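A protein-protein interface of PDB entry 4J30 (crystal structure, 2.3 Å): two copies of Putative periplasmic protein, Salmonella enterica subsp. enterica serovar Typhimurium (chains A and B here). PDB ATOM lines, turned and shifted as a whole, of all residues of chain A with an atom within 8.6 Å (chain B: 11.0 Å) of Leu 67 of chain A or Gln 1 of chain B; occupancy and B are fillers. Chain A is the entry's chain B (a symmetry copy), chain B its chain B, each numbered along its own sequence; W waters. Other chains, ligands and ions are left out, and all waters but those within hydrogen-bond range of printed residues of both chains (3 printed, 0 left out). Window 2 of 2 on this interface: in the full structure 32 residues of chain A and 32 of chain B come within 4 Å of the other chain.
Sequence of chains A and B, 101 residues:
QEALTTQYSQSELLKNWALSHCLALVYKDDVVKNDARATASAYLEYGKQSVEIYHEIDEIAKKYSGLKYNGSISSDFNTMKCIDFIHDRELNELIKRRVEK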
ATOM      1  N   VAL A  26     -33.590 -32.966 -23.583  1.00  0.00           N
ATOM      2  CA  VAL A  26     -32.324 -33.579 -23.139  1.00  0.00           C
ATOM      3  C   VAL A  26     -32.459 -34.879 -22.346  1.00  0.00           C
ATOM      4  O   VAL A  26     -31.572 -35.730 -22.394  1.00  0.00           O
ATOM      5  CB  VAL A  26     -31.410 -32.583 -22.352  1.00  0.00           C
ATOM      6  CG1 VAL A  26     -30.987 -31.413 -23.243  1.00  0.00           C
ATOM      7  CG2 VAL A  26     -32.083 -32.096 -21.066  1.00  0.00           C
ATOM      8  N   ILE A  60     -33.090 -22.652 -31.127  1.00  0.00           N
ATOM      9  CA  ILE A  60     -31.993 -22.206 -30.276  1.00  0.00           C
ATOM     10  C   ILE A  60     -31.691 -23.268 -29.226  1.00  0.00           C
ATOM     11  O   ILE A  60     -30.527 -23.516 -28.909  1.00  0.00           O
ATOM     12  CB  ILE A  60     -32.271 -20.834 -29.609  1.00  0.00           C
ATOM     13  CG1 ILE A  60     -32.563 -19.775 -30.675  1.00  0.00           C
ATOM     14  CG2 ILE A  60     -31.074 -20.413 -28.721  1.00  0.00           C
ATOM     15  CD1 ILE A  60     -33.040 -18.436 -30.120  1.00  0.00           C
ATOM     16  N   ALA A  61     -32.746 -23.909 -28.714  1.00  0.00           N
ATOM     17  CA  ALA A  61     -32.610 -24.972 -27.707  1.00  0.00           C
ATOM     18  C   ALA A  61     -31.746 -26.117 -28.215  1.00  0.00           C
ATOM     19  O   ALA A  61     -30.966 -26.679 -27.446  1.00  0.00           O
ATOM     20  CB  ALA A  61     -33.993 -25.497 -27.271  1.00  0.00           C
ATOM     21  N   LYS A  62     -31.885 -26.441 -29.506  1.00  0.00           N
ATOM     22  CA  LYS A  62     -31.159 -27.552 -30.138  1.00  0.00           C
ATOM     23  C   LYS A  62     -29.666 -27.295 -30.285  1.00  0.00           C
ATOM     24  O   LYS A  62     -28.893 -28.229 -30.483  1.00  0.00           O
ATOM     25  CB  LYS A  62     -31.766 -27.917 -31.502  1.00  0.00           C
ATOM     26  CG  LYS A  62     -33.190 -28.484 -31.418  1.00  0.00           C
ATOM     27  CD  LYS A  62     -33.463 -29.482 -32.536  1.00  0.00           C
ATOM     28  CE  LYS A  62     -34.966 -29.712 -32.788  1.00  0.00           C
ATOM     29  NZ  LYS A  62     -35.766 -30.104 -31.576  1.00  0.00           N
ATOM     30  N   LYS A  63     -29.263 -26.029 -30.199  1.00  0.00           N
ATOM     31  CA  LYS A  63     -27.845 -25.666 -30.188  1.00  0.00           C
ATOM     32  C   LYS A  63     -27.197 -25.955 -28.829  1.00  0.00           C
ATOM     33  O   LYS A  63     -25.973 -25.969 -28.722  1.00  0.00           O
ATOM     34  CB  LYS A  63     -27.658 -24.197 -30.574  1.00  0.00           C
ATOM     35  CG  LYS A  63     -28.310 -23.850 -31.910  1.00  0.00           C
ATOM     36  CD  LYS A  63     -27.735 -22.597 -32.552  1.00  0.00           C
ATOM     37  CE  LYS A  63     -28.275 -21.334 -31.917  1.00  0.00           C
ATOM     38  NZ  LYS A  63     -28.400 -20.282 -32.966  1.00  0.00           N
ATOM     39  N   TYR A  64     -28.021 -26.180 -27.805  1.00  0.00           N
ATOM     40  CA  TYR A  64     -27.546 -26.535 -26.464  1.00  0.00           C
ATOM     41  C   TYR A  64     -27.770 -28.019 -26.182  1.00  0.00           C
ATOM     42  O   TYR A  64     -26.900 -28.681 -25.625  1.00  0.00           O
ATOM     43  CB  TYR A  64     -28.220 -25.665 -25.388  1.00  0.00           C
ATOM     44  CG  TYR A  64     -27.692 -24.249 -25.377  1.00  0.00           C
ATOM     45  CD1 TYR A  64     -26.642 -23.889 -24.527  1.00  0.00           C
ATOM     46  CD2 TYR A  64     -28.217 -23.277 -26.241  1.00  0.00           C
ATOM     47  CE1 TYR A  64     -26.123 -22.594 -24.528  1.00  0.00           C
ATOM     48  CE2 TYR A  64     -27.705 -21.970 -26.253  1.00  0.00           C
ATOM     49  CZ  TYR A  64     -26.658 -21.638 -25.390  1.00  0.00           C
ATOM     50  OH  TYR A  64     -26.140 -20.356 -25.387  1.00  0.00           O
ATOM     51  N   SER A  65     -28.931 -28.532 -26.590  1.00  0.00           N
ATOM     52  CA  SER A  65     -29.290 -29.925 -26.359  1.00  0.00           C
ATOM     53  C   SER A  65     -28.355 -30.892 -27.097  1.00  0.00           C
ATOM     54  O   SER A  65     -28.203 -32.032 -26.674  1.00  0.00           O
ATOM     55  CB  SER A  65     -30.755 -30.187 -26.734  1.00  0.00           C
ATOM     56  OG  SER A  65     -30.916 -30.254 -28.141  1.00  0.00           O
ATOM     57  N   GLY A  66     -27.723 -30.425 -28.175  1.00  0.00           N
ATOM     58  CA  GLY A  66     -26.766 -31.224 -28.949  1.00  0.00           C
ATOM     59  C   GLY A  66     -25.330 -31.200 -28.428  1.00  0.00           C
ATOM     60  O   GLY A  66     -24.483 -31.950 -28.903  1.00  0.00           O
ATOM     61  N   LEU A  67     -25.054 -30.338 -27.449  1.00  0.00           N
ATOM     62  CA  LEU A  67     -23.701 -30.164 -26.917  1.00  0.00           C
ATOM     63  C   LEU A  67     -23.269 -31.394 -26.136  1.00  0.00           C
ATOM     64  O   LEU A  67     -24.102 -32.098 -25.567  1.00  0.00           O
ATOM     65  CB  LEU A  67     -23.629 -28.931 -26.005  1.00  0.00           C
ATOM     66  CG  LEU A  67     -23.906 -27.533 -26.577  1.00  0.00           C
ATOM     67  CD1 LEU A  67     -23.882 -26.466 -25.486  1.00  0.00           C
ATOM     68  CD2 LEU A  67     -22.944 -27.175 -27.703  1.00  0.00           C
ATOM     69  N   LYS A  68     -21.966 -31.660 -26.127  1.00  0.00           N
ATOM     70  CA  LYS A  68     -21.405 -32.644 -25.213  1.00  0.00           C
ATOM     71  C   LYS A  68     -20.684 -31.927 -24.086  1.00  0.00           C
ATOM     72  O   LYS A  68     -19.700 -31.219 -24.311  1.00  0.00           O
ATOM     73  CB  LYS A  68     -20.465 -33.632 -25.925  1.00  0.00           C
ATOM     74  CG  LYS A  68     -21.131 -34.472 -27.031  1.00  0.00           C
ATOM     75  CD  LYS A  68     -22.464 -35.116 -26.578  1.00  0.00           C
ATOM     76  CE  LYS A  68     -23.057 -35.986 -27.697  1.00  0.00           C
ATOM     77  NZ  LYS A  68     -24.555 -36.080 -27.608  1.00  0.00           N
ATOM     78  N   TYR A  69     -21.196 -32.116 -22.873  1.00  0.00           N
ATOM     79  CA  TYR A  69     -20.599 -31.561 -21.660  1.00  0.00           C
ATOM     80  C   TYR A  69     -19.906 -32.657 -20.845  1.00  0.00           C
ATOM     81  O   TYR A  69     -20.476 -33.722 -20.630  1.00  0.00           O
ATOM     82  CB  TYR A  69     -21.678 -30.905 -20.795  1.00  0.00           C
ATOM     83  CG  TYR A  69     -22.114 -29.518 -21.211  1.00  0.00           C
ATOM     84  CD1 TYR A  69     -23.170 -28.891 -20.550  1.00  0.00           C
ATOM     85  CD2 TYR A  69     -21.474 -28.823 -22.250  1.00  0.00           C
ATOM     86  CE1 TYR A  69     -23.579 -27.614 -20.891  1.00  0.00           C
ATOM     87  CE2 TYR A  69     -21.882 -27.534 -22.611  1.00  0.00           C
ATOM     88  CZ  TYR A  69     -22.933 -26.937 -21.922  1.00  0.00           C
ATOM     89  OH  TYR A  69     -23.344 -25.665 -22.241  1.00  0.00           O
ATOM     90  N   ASN A  70     -18.692 -32.371 -20.377  1.00  0.00           N
ATOM     91  CA  ASN A  70     -17.889 -33.329 -19.602  1.00  0.00           C
ATOM     92  C   ASN A  70     -17.420 -32.775 -18.252  1.00  0.00           C
ATOM     93  O   ASN A  70     -17.371 -31.565 -18.057  1.00  0.00           O
ATOM     94  CB  ASN A  70     -16.670 -33.760 -20.426  1.00  0.00           C
ATOM     95  CG  ASN A  70     -17.062 -34.459 -21.719  1.00  0.00           C
ATOM     96  OD1 ASN A  70     -17.331 -35.668 -21.726  1.00  0.00           O
ATOM     97  ND2 ASN A  70     -17.084 -33.705 -22.823  1.00  0.00           N
ATOM     98  N   GLY A  71     -17.072 -33.668 -17.329  1.00  0.00           N
ATOM     99  CA  GLY A  71     -16.619 -33.272 -16.006  1.00  0.00           C
ATOM    100  C   GLY A  71     -15.735 -34.305 -15.354  1.00  0.00           C
ATOM    101  O   GLY A  71     -15.500 -35.370 -15.922  1.00  0.00           O
ATOM    102  N   ASP A  76     -23.546 -36.710 -18.113  1.00  0.00           N
ATOM    103  CA  ASP A  76     -23.696 -36.038 -19.395  1.00  0.00           C
ATOM    104  C   ASP A  76     -24.035 -34.563 -19.191  1.00  0.00           C
ATOM    105  O   ASP A  76     -24.001 -33.780 -20.139  1.00  0.00           O
ATOM    106  CB  ASP A  76     -24.789 -36.712 -20.235  1.00  0.00           C
ATOM    107  CG  ASP A  76     -24.381 -38.076 -20.738  1.00  0.00           C
ATOM    108  OD1 ASP A  76     -23.179 -38.331 -20.939  1.00  0.00           O
ATOM    109  OD2 ASP A  76     -25.269 -38.914 -20.932  1.00  0.00           O
ATOM    110  N   PHE A  77     -24.363 -34.196 -17.955  1.00  0.00           N
ATOM    111  CA  PHE A  77     -24.716 -32.816 -17.594  1.00  0.00           C
ATOM    112  C   PHE A  77     -25.839 -32.248 -18.494  1.00  0.00           C
ATOM    113  O   PHE A  77     -25.781 -31.093 -18.933  1.00  0.00           O
ATOM    114  CB  PHE A  77     -23.488 -31.901 -17.601  1.00  0.00           C
ATOM    115  CG  PHE A  77     -22.445 -32.248 -16.555  1.00  0.00           C
ATOM    116  CD1 PHE A  77     -22.618 -31.876 -15.225  1.00  0.00           C
ATOM    117  CD2 PHE A  77     -21.274 -32.915 -16.916  1.00  0.00           C
ATOM    118  CE1 PHE A  77     -21.654 -32.189 -14.267  1.00  0.00           C
ATOM    119  CE2 PHE A  77     -20.307 -33.226 -15.963  1.00  0.00           C
ATOM    120  CZ  PHE A  77     -20.498 -32.858 -14.633  1.00  0.00           C
ATOM    121  N   ASN A  78     -26.847 -33.076 -18.763  1.00  0.00           N
ATOM    122  CA  ASN A  78     -27.980 -32.670 -19.585  1.00  0.00           C
ATOM    123  C   ASN A  78     -28.723 -31.458 -19.014  1.00  0.00           C
ATOM    124  O   ASN A  78     -29.022 -30.520 -19.744  1.00  0.00           O
ATOM    125  CB  ASN A  78     -28.937 -33.841 -19.777  1.00  0.00           C
ATOM    126  CG  ASN A  78     -28.381 -34.891 -20.714  1.00  0.00           C
ATOM    127  OD1 ASN A  78     -27.782 -34.567 -21.747  1.00  0.00           O
ATOM    128  ND2 ASN A  78     -28.576 -36.164 -20.360  1.00  0.00           N
ATOM    129  N   MET A  80     -27.675 -29.104 -17.278  1.00  0.00           N
ATOM    130  CA  MET A  80     -26.819 -27.930 -17.418  1.00  0.00           C
ATOM    131  C   MET A  80     -26.894 -27.293 -18.798  1.00  0.00           C
ATOM    132  O   MET A  80     -26.733 -26.084 -18.940  1.00  0.00           O
ATOM    133  CB  MET A  80     -25.380 -28.348 -17.124  1.00  0.00           C
ATOM    134  CG  MET A  80     -24.384 -27.229 -17.155  1.00  0.00           C
ATOM    135  SD  MET A  80     -22.597 -27.845 -16.756  1.00  0.00           S
ATOM    136  CE  MET A  80     -22.780 -28.061 -14.832  1.00  0.00           C
ATOM    137  N   LYS A  81     -27.108 -28.109 -19.825  1.00  0.00           N
ATOM    138  CA  LYS A  81     -27.308 -27.589 -21.169  1.00  0.00           C
ATOM    139  C   LYS A  81     -28.500 -26.635 -21.179  1.00  0.00           C
ATOM    140  O   LYS A  81     -28.437 -25.563 -21.764  1.00  0.00           O
ATOM    141  CB  LYS A  81     -27.516 -28.735 -22.167  1.00  0.00           C
ATOM    142  CG  LYS A  81     -26.302 -29.670 -22.277  1.00  0.00           C
ATOM    143  CD  LYS A  81     -26.692 -31.027 -22.819  1.00  0.00           C
ATOM    144  CE  LYS A  81     -25.521 -31.983 -22.754  1.00  0.00           C
ATOM    145  NZ  LYS A  81     -25.836 -33.318 -23.329  1.00  0.00           N
ATOM    146  N   CYS A  82     -29.571 -27.027 -20.494  1.00  0.00           N
ATOM    147  CA  CYS A  82     -30.788 -26.233 -20.445  1.00  0.00           C
ATOM    148  C   CYS A  82     -30.674 -24.987 -19.569  1.00  0.00           C
ATOM    149  O   CYS A  82     -31.305 -23.968 -19.853  1.00  0.00           O
ATOM    150  CB  CYS A  82     -31.967 -27.103 -20.024  1.00  0.00           C
ATOM    151  SG  CYS A  82     -32.314 -28.341 -21.246  1.00  0.00           S
ATOM    152  N   ASP A  84     -27.659 -23.386 -19.160  1.00  0.00           N
ATOM    153  CA  ASP A  84     -26.890 -22.558 -20.079  1.00  0.00           C
ATOM    154  C   ASP A  84     -27.789 -21.950 -21.171  1.00  0.00           C
ATOM    155  O   ASP A  84     -27.692 -20.766 -21.469  1.00  0.00           O
ATOM    156  CB  ASP A  84     -25.734 -23.359 -20.682  1.00  0.00           C
ATOM    157  CG  ASP A  84     -24.618 -23.611 -19.684  1.00  0.00           C
ATOM    158  OD1 ASP A  84     -24.688 -23.082 -18.545  1.00  0.00           O
ATOM    159  OD2 ASP A  84     -23.663 -24.339 -20.039  1.00  0.00           O
ATOM    160  N   PHE A  85     -28.680 -22.768 -21.727  1.00  0.00           N
ATOM    161  CA  PHE A  85     -29.654 -22.316 -22.731  1.00  0.00           C
ATOM    162  C   PHE A  85     -30.495 -21.098 -22.310  1.00  0.00           C
ATOM    163  O   PHE A  85     -30.581 -20.135 -23.063  1.00  0.00           O
ATOM    164  CB  PHE A  85     -30.544 -23.485 -23.186  1.00  0.00           C
ATOM    165  CG  PHE A  85     -31.728 -23.074 -24.027  1.00  0.00           C
ATOM    166  CD1 PHE A  85     -31.566 -22.275 -25.165  1.00  0.00           C
ATOM    167  CD2 PHE A  85     -33.011 -23.510 -23.696  1.00  0.00           C
ATOM    168  CE1 PHE A  85     -32.667 -21.903 -25.940  1.00  0.00           C
ATOM    169  CE2 PHE A  85     -34.107 -23.146 -24.474  1.00  0.00           C
ATOM    170  CZ  PHE A  85     -33.933 -22.342 -25.594  1.00  0.00           C
ATOM    171  N   GLN B   1     -17.175 -29.501 -25.555  1.00  0.00           N
ATOM    172  CA  GLN B   1     -17.593 -28.141 -25.128  1.00  0.00           C
ATOM    173  C   GLN B   1     -17.488 -28.021 -23.612  1.00  0.00           C
ATOM    174  O   GLN B   1     -17.992 -28.875 -22.874  1.00  0.00           O
ATOM    175  CB  GLN B   1     -19.039 -27.844 -25.570  1.00  0.00           C
ATOM    176  CG  GLN B   1     -19.228 -27.422 -27.039  1.00  0.00           C
ATOM    177  CD  GLN B   1     -19.723 -28.553 -27.970  1.00  0.00           C
ATOM    178  OE1 GLN B   1     -20.112 -29.641 -27.519  1.00  0.00           O
ATOM    179  NE2 GLN B   1     -19.722 -28.281 -29.277  1.00  0.00           N
ATOM    180  N   GLU B   2     -16.833 -26.963 -23.141  1.00  0.00           N
ATOM    181  CA  GLU B   2     -16.952 -26.606 -21.737  1.00  0.00           C
ATOM    182  C   GLU B   2     -18.251 -25.817 -21.567  1.00  0.00           C
ATOM    183  O   GLU B   2     -18.560 -24.937 -22.376  1.00  0.00           O
ATOM    184  CB  GLU B   2     -15.746 -25.800 -21.237  1.00  0.00           C
ATOM    185  CG  GLU B   2     -15.748 -25.603 -19.712  1.00  0.00           C
ATOM    186  CD  GLU B   2     -14.533 -24.849 -19.184  1.00  0.00           C
ATOM    187  OE1 GLU B   2     -14.705 -23.995 -18.289  1.00  0.00           O
ATOM    188  OE2 GLU B   2     -13.408 -25.104 -19.646  1.00  0.00           O
ATOM    189  N   ALA B   3     -19.015 -26.149 -20.528  1.00  0.00           N
ATOM    190  CA  ALA B   3     -20.210 -25.387 -20.169  1.00  0.00           C
ATOM    191  C   ALA B   3     -19.858 -23.957 -19.760  1.00  0.00           C
ATOM    192  O   ALA B   3     -18.677 -23.596 -19.681  1.00  0.00           O
ATOM    193  CB  ALA B   3     -20.976 -26.085 -19.050  1.00  0.00           C
ATOM    194  N   LEU B   4     -20.887 -23.158 -19.490  1.00  0.00           N
ATOM    195  CA  LEU B   4     -20.725 -21.749 -19.144  1.00  0.00           C
ATOM    196  C   LEU B   4     -20.518 -21.510 -17.662  1.00  0.00           C
ATOM    197  O   LEU B   4     -20.515 -20.362 -17.220  1.00  0.00           O
ATOM    198  CB  LEU B   4     -21.935 -20.946 -19.621  1.00  0.00           C
ATOM    199  CG  LEU B   4     -22.252 -21.062 -21.110  1.00  0.00           C
ATOM    200  CD1 LEU B   4     -23.488 -20.236 -21.433  1.00  0.00           C
ATOM    201  CD2 LEU B   4     -21.057 -20.635 -21.975  1.00  0.00           C
ATOM    202  N   THR B   5     -20.319 -22.596 -16.910  1.00  0.00           N
ATOM    203  CA  THR B   5     -20.275 -22.589 -15.445  1.00  0.00           C
ATOM    204  C   THR B   5     -19.419 -21.482 -14.804  1.00  0.00           C
ATOM    205  O   THR B   5     -19.837 -20.880 -13.815  1.00  0.00           O
ATOM    206  CB  THR B   5     -19.826 -23.970 -14.906  1.00  0.00           C
ATOM    207  OG1 THR B   5     -20.308 -24.998 -15.782  1.00  0.00           O
ATOM    208  CG2 THR B   5     -20.376 -24.214 -13.491  1.00  0.00           C
ATOM    209  N   THR B   6     -18.237 -21.215 -15.363  1.00  0.00           N
ATOM    210  CA  THR B   6     -17.335 -20.182 -14.822  1.00  0.00           C
ATOM    211  C   THR B   6     -17.750 -18.738 -15.123  1.00  0.00           C
ATOM    212  O   THR B   6     -17.131 -17.800 -14.613  1.00  0.00           O
ATOM    213  CB  THR B   6     -15.891 -20.344 -15.351  1.00  0.00           C
ATOM    214  OG1 THR B   6     -15.902 -20.390 -16.784  1.00  0.00           O
ATOM    215  CG2 THR B   6     -15.258 -21.602 -14.803  1.00  0.00           C
ATOM    216  N   GLN B   7     -18.773 -18.559 -15.955  1.00  0.00           N
ATOM    217  CA  GLN B   7     -19.206 -17.227 -16.372  1.00  0.00           C
ATOM    218  C   GLN B   7     -20.281 -16.654 -15.450  1.00  0.00           C
ATOM    219  O   GLN B   7     -20.546 -15.453 -15.466  1.00  0.00           O
ATOM    220  CB  GLN B   7     -19.692 -17.248 -17.833  1.00  0.00           C
ATOM    221  CG  GLN B   7     -18.597 -17.620 -18.823  1.00  0.00           C
ATOM    222  CD  GLN B   7     -19.074 -17.624 -20.268  1.00  0.00           C
ATOM    223  OE1 GLN B   7     -20.094 -17.013 -20.607  1.00  0.00           O
ATOM    224  NE2 GLN B   7     -18.331 -18.308 -21.133  1.00  0.00           N
ATOM    225  N   TYR B   8     -20.883 -17.518 -14.637  1.00  0.00           N
ATOM    226  CA  TYR B   8     -21.959 -17.090 -13.739  1.00  0.00           C
ATOM    227  C   TYR B   8     -21.472 -16.321 -12.510  1.00  0.00           C
ATOM    228  O   TYR B   8     -20.473 -16.693 -11.855  1.00  0.00           O
ATOM    229  CB  TYR B   8     -22.836 -18.275 -13.310  1.00  0.00           C
ATOM    230  CG  TYR B   8     -23.545 -18.952 -14.459  1.00  0.00           C
ATOM    231  CD1 TYR B   8     -24.519 -18.275 -15.192  1.00  0.00           C
ATOM    232  CD2 TYR B   8     -23.245 -20.270 -14.811  1.00  0.00           C
ATOM    233  CE1 TYR B   8     -25.171 -18.883 -16.253  1.00  0.00           C
ATOM    234  CE2 TYR B   8     -23.900 -20.897 -15.872  1.00  0.00           C
ATOM    235  CZ  TYR B   8     -24.861 -20.191 -16.587  1.00  0.00           C
ATOM    236  OH  TYR B   8     -25.516 -20.778 -17.641  1.00  0.00           O
ATOM    237  N   ASP B  35     -28.142 -36.868 -12.947  1.00  0.00           N
ATOM    238  CA  ASP B  35     -27.752 -35.803 -13.856  1.00  0.00           C
ATOM    239  C   ASP B  35     -27.960 -34.439 -13.208  1.00  0.00           C
ATOM    240  O   ASP B  35     -27.037 -33.622 -13.179  1.00  0.00           O
ATOM    241  CB  ASP B  35     -28.551 -35.922 -15.152  1.00  0.00           C
ATOM    242  CG  ASP B  35     -28.048 -35.002 -16.229  1.00  0.00           C
ATOM    243  OD1 ASP B  35     -27.305 -35.484 -17.104  1.00  0.00           O
ATOM    244  OD2 ASP B  35     -28.388 -33.802 -16.198  1.00  0.00           O
ATOM    245  N   TYR B  43     -22.381 -26.055  -9.766  1.00  0.00           N
ATOM    246  CA  TYR B  43     -22.667 -24.703  -9.256  1.00  0.00           C
ATOM    247  C   TYR B  43     -22.208 -24.518  -7.805  1.00  0.00           C
ATOM    248  O   TYR B  43     -21.759 -23.425  -7.424  1.00  0.00           O
ATOM    249  CB  TYR B  43     -24.158 -24.343  -9.435  1.00  0.00           C
ATOM    250  CG  TYR B  43     -24.578 -24.467 -10.887  1.00  0.00           C
ATOM    251  CD1 TYR B  43     -23.859 -23.799 -11.890  1.00  0.00           C
ATOM    252  CD2 TYR B  43     -25.652 -25.270 -11.266  1.00  0.00           C
ATOM    253  CE1 TYR B  43     -24.197 -23.923 -13.240  1.00  0.00           C
ATOM    254  CE2 TYR B  43     -26.006 -25.402 -12.642  1.00  0.00           C
ATOM    255  CZ  TYR B  43     -25.273 -24.720 -13.608  1.00  0.00           C
ATOM    256  OH  TYR B  43     -25.576 -24.825 -14.944  1.00  0.00           O
HETATM  257  O   HOH W   1     -26.282 -37.762 -17.153  1.00  0.00           O
HETATM  258  O   HOH W   2     -29.947 -37.156 -18.060  1.00  0.00           O
HETATM  259  O   HOH W   3     -23.479 -24.119 -16.391  1.00  0.00           O
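No position is printed for both chains. Of the 13 pairs that touch across the chains among the printed residues, none has its exchanged pair printed and touching as well.
Among the printed residues, merely in contact across the chains: Leu 67 of chain A with Gln 1 of chain B (3.5 Å), Tyr 69 of chain A with Gln 1 of chain B (3.5 Å), Tyr 69 of chain A with Ala 3 of chain B (3.5 Å), Asp 76 of chain A with Asp 35 of chain B (3.99 Å), Met 80 of chain A with Ala 3 of chain B (3.3 Å), Met 80 of chain A with Tyr 43 of chain B (3.5 Å) and Asp 84 of chain A with Ala 3 of chain B (3.4 Å).
Water W1 lies within hydrogen-bond range of OD1 of Asp 35 of chain B (2.5 Å) and N of Asp 76 of chain A (3.1 Å). Water W3 lies within hydrogen-bond range of OH of Tyr 43 of chain B, OD1 of Asp 84 of chain A and OG1 of Thr 5 of chain B. Water W2 bridges the side-chain amide nitrogen (ND2) of Asn 78 of chain A (2.9 Å) and the side-chain carboxylate (OD1) of Asp 35 of chain B (3.3 Å).
The backbone carbonyl oxygen (O) of Leu 67 of chain A lies within hydrogen-bond range of the side-chain amino group (NZ) of Lys 81 of chain A, at 3.1 Å. OH of Tyr 69 of chain A lies within hydrogen-bond range of OD2 of Asp 84 of chain A. The side-chain amide oxygen (OD1) of Asn 78 of chain A lies within hydrogen-bond range of the side-chain amino group (NZ) of Lys 81 of chain A, at 2.8 Å.
N of Lys 68 of chain A lies within hydrogen-bond range of OE1 of Gln 1 of chain B, at 3.1 Å. N of Leu 4 of chain B lies within hydrogen-bond range of OD2 of Asp 84 of chain A, at 3.1 Å. OG1 of Thr 5 of chain B is in hydrogen-bond range of SD of Met 80 of chain A, at 3.8 Å. The side-chain hydroxyl of Tyr 8 of chain B sits at hydrogen-bond distance from the side-chain carboxylate of Asp 84 of chain A, 2.6 Å away. OD1 of Asp 35 of chain B sits at hydrogen-bond distance from N of Phe 77 of chain A (3.3 Å). OD1 of Asp 35 of chain B is in hydrogen-bond range of N of Asn 78 of chain A, 3.0 Å away.
No residue of chain B comes within 4 Å of Tyr 64 of chain A. No residue of chain B comes within 4 Å of Ser 65 of chain A. No residue of chain B comes within 4 Å of Gly 66 of chain A. Of chain B, only Gln 1 (3.5 Å) comes within 4 Å of Leu 67 of chain A. Lys 68 of chain A touches just one residue of chain B: Gln 1 (3.1 Å). Tyr 69 of chain A touches two residues of chain B. No residue of chain B comes within 4 Å of Asn 70 of chain A. Printed residues of chain B within 4 Å of Asp 76 of chain A: Asp 35 (3.99 Å). Of the printed residues of chain B, Met 80 of chain A touches Ala 3 (3.3 Å), Thr 5 (3.8 Å) and Tyr 43 (3.5 Å). No residue of chain B comes within 4 Å of Lys 81 of chain A. Of the printed residues of chain B, Asp 84 of chain A touches Ala 3, Leu 4 and Tyr 8. Printed residues of chain A within 4 Å of Gln 1 of chain B: Leu 67 (3.5 Å), Lys 68 (3.1 Å) and Tyr 69 (3.5 Å). Of the printed residues of chain A, Ala 3 of chain B touches Tyr 69 (3.5 Å), Met 80 (3.3 Å) and Asp 84 (3.4 Å). Printed residues of chain A within 4 Å of Asp 35 of chain B: Asp 76, Phe 77 and Asn 78. The nearest residue of chain B that does not touch Leu 67 of chain A is Glu 2 of chain B (6.4 Å). The nearest residue of chain A that does not touch Gln 1 of chain B is Asn 70 of chain A (4.4 Å). The nearest printed residue of chain B that does not touch Asp 84 of chain A is Tyr 43 of chain B (4.1 Å).
Hydrophobic or aromatic side chains of chain B within 4 Å of the printed part of chain A: Ala 3, Leu 4, Tyr 8 and Tyr 43. Of the 21 printed residues of chain A, 8 touch a printed residue of chain B. Among the printed residues, 13 pairs touch across the chains. Among the printed residues, no Asp or Glu carboxylate lies within 4 Å of a Lys or Arg side-chain nitrogen of the other chain.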
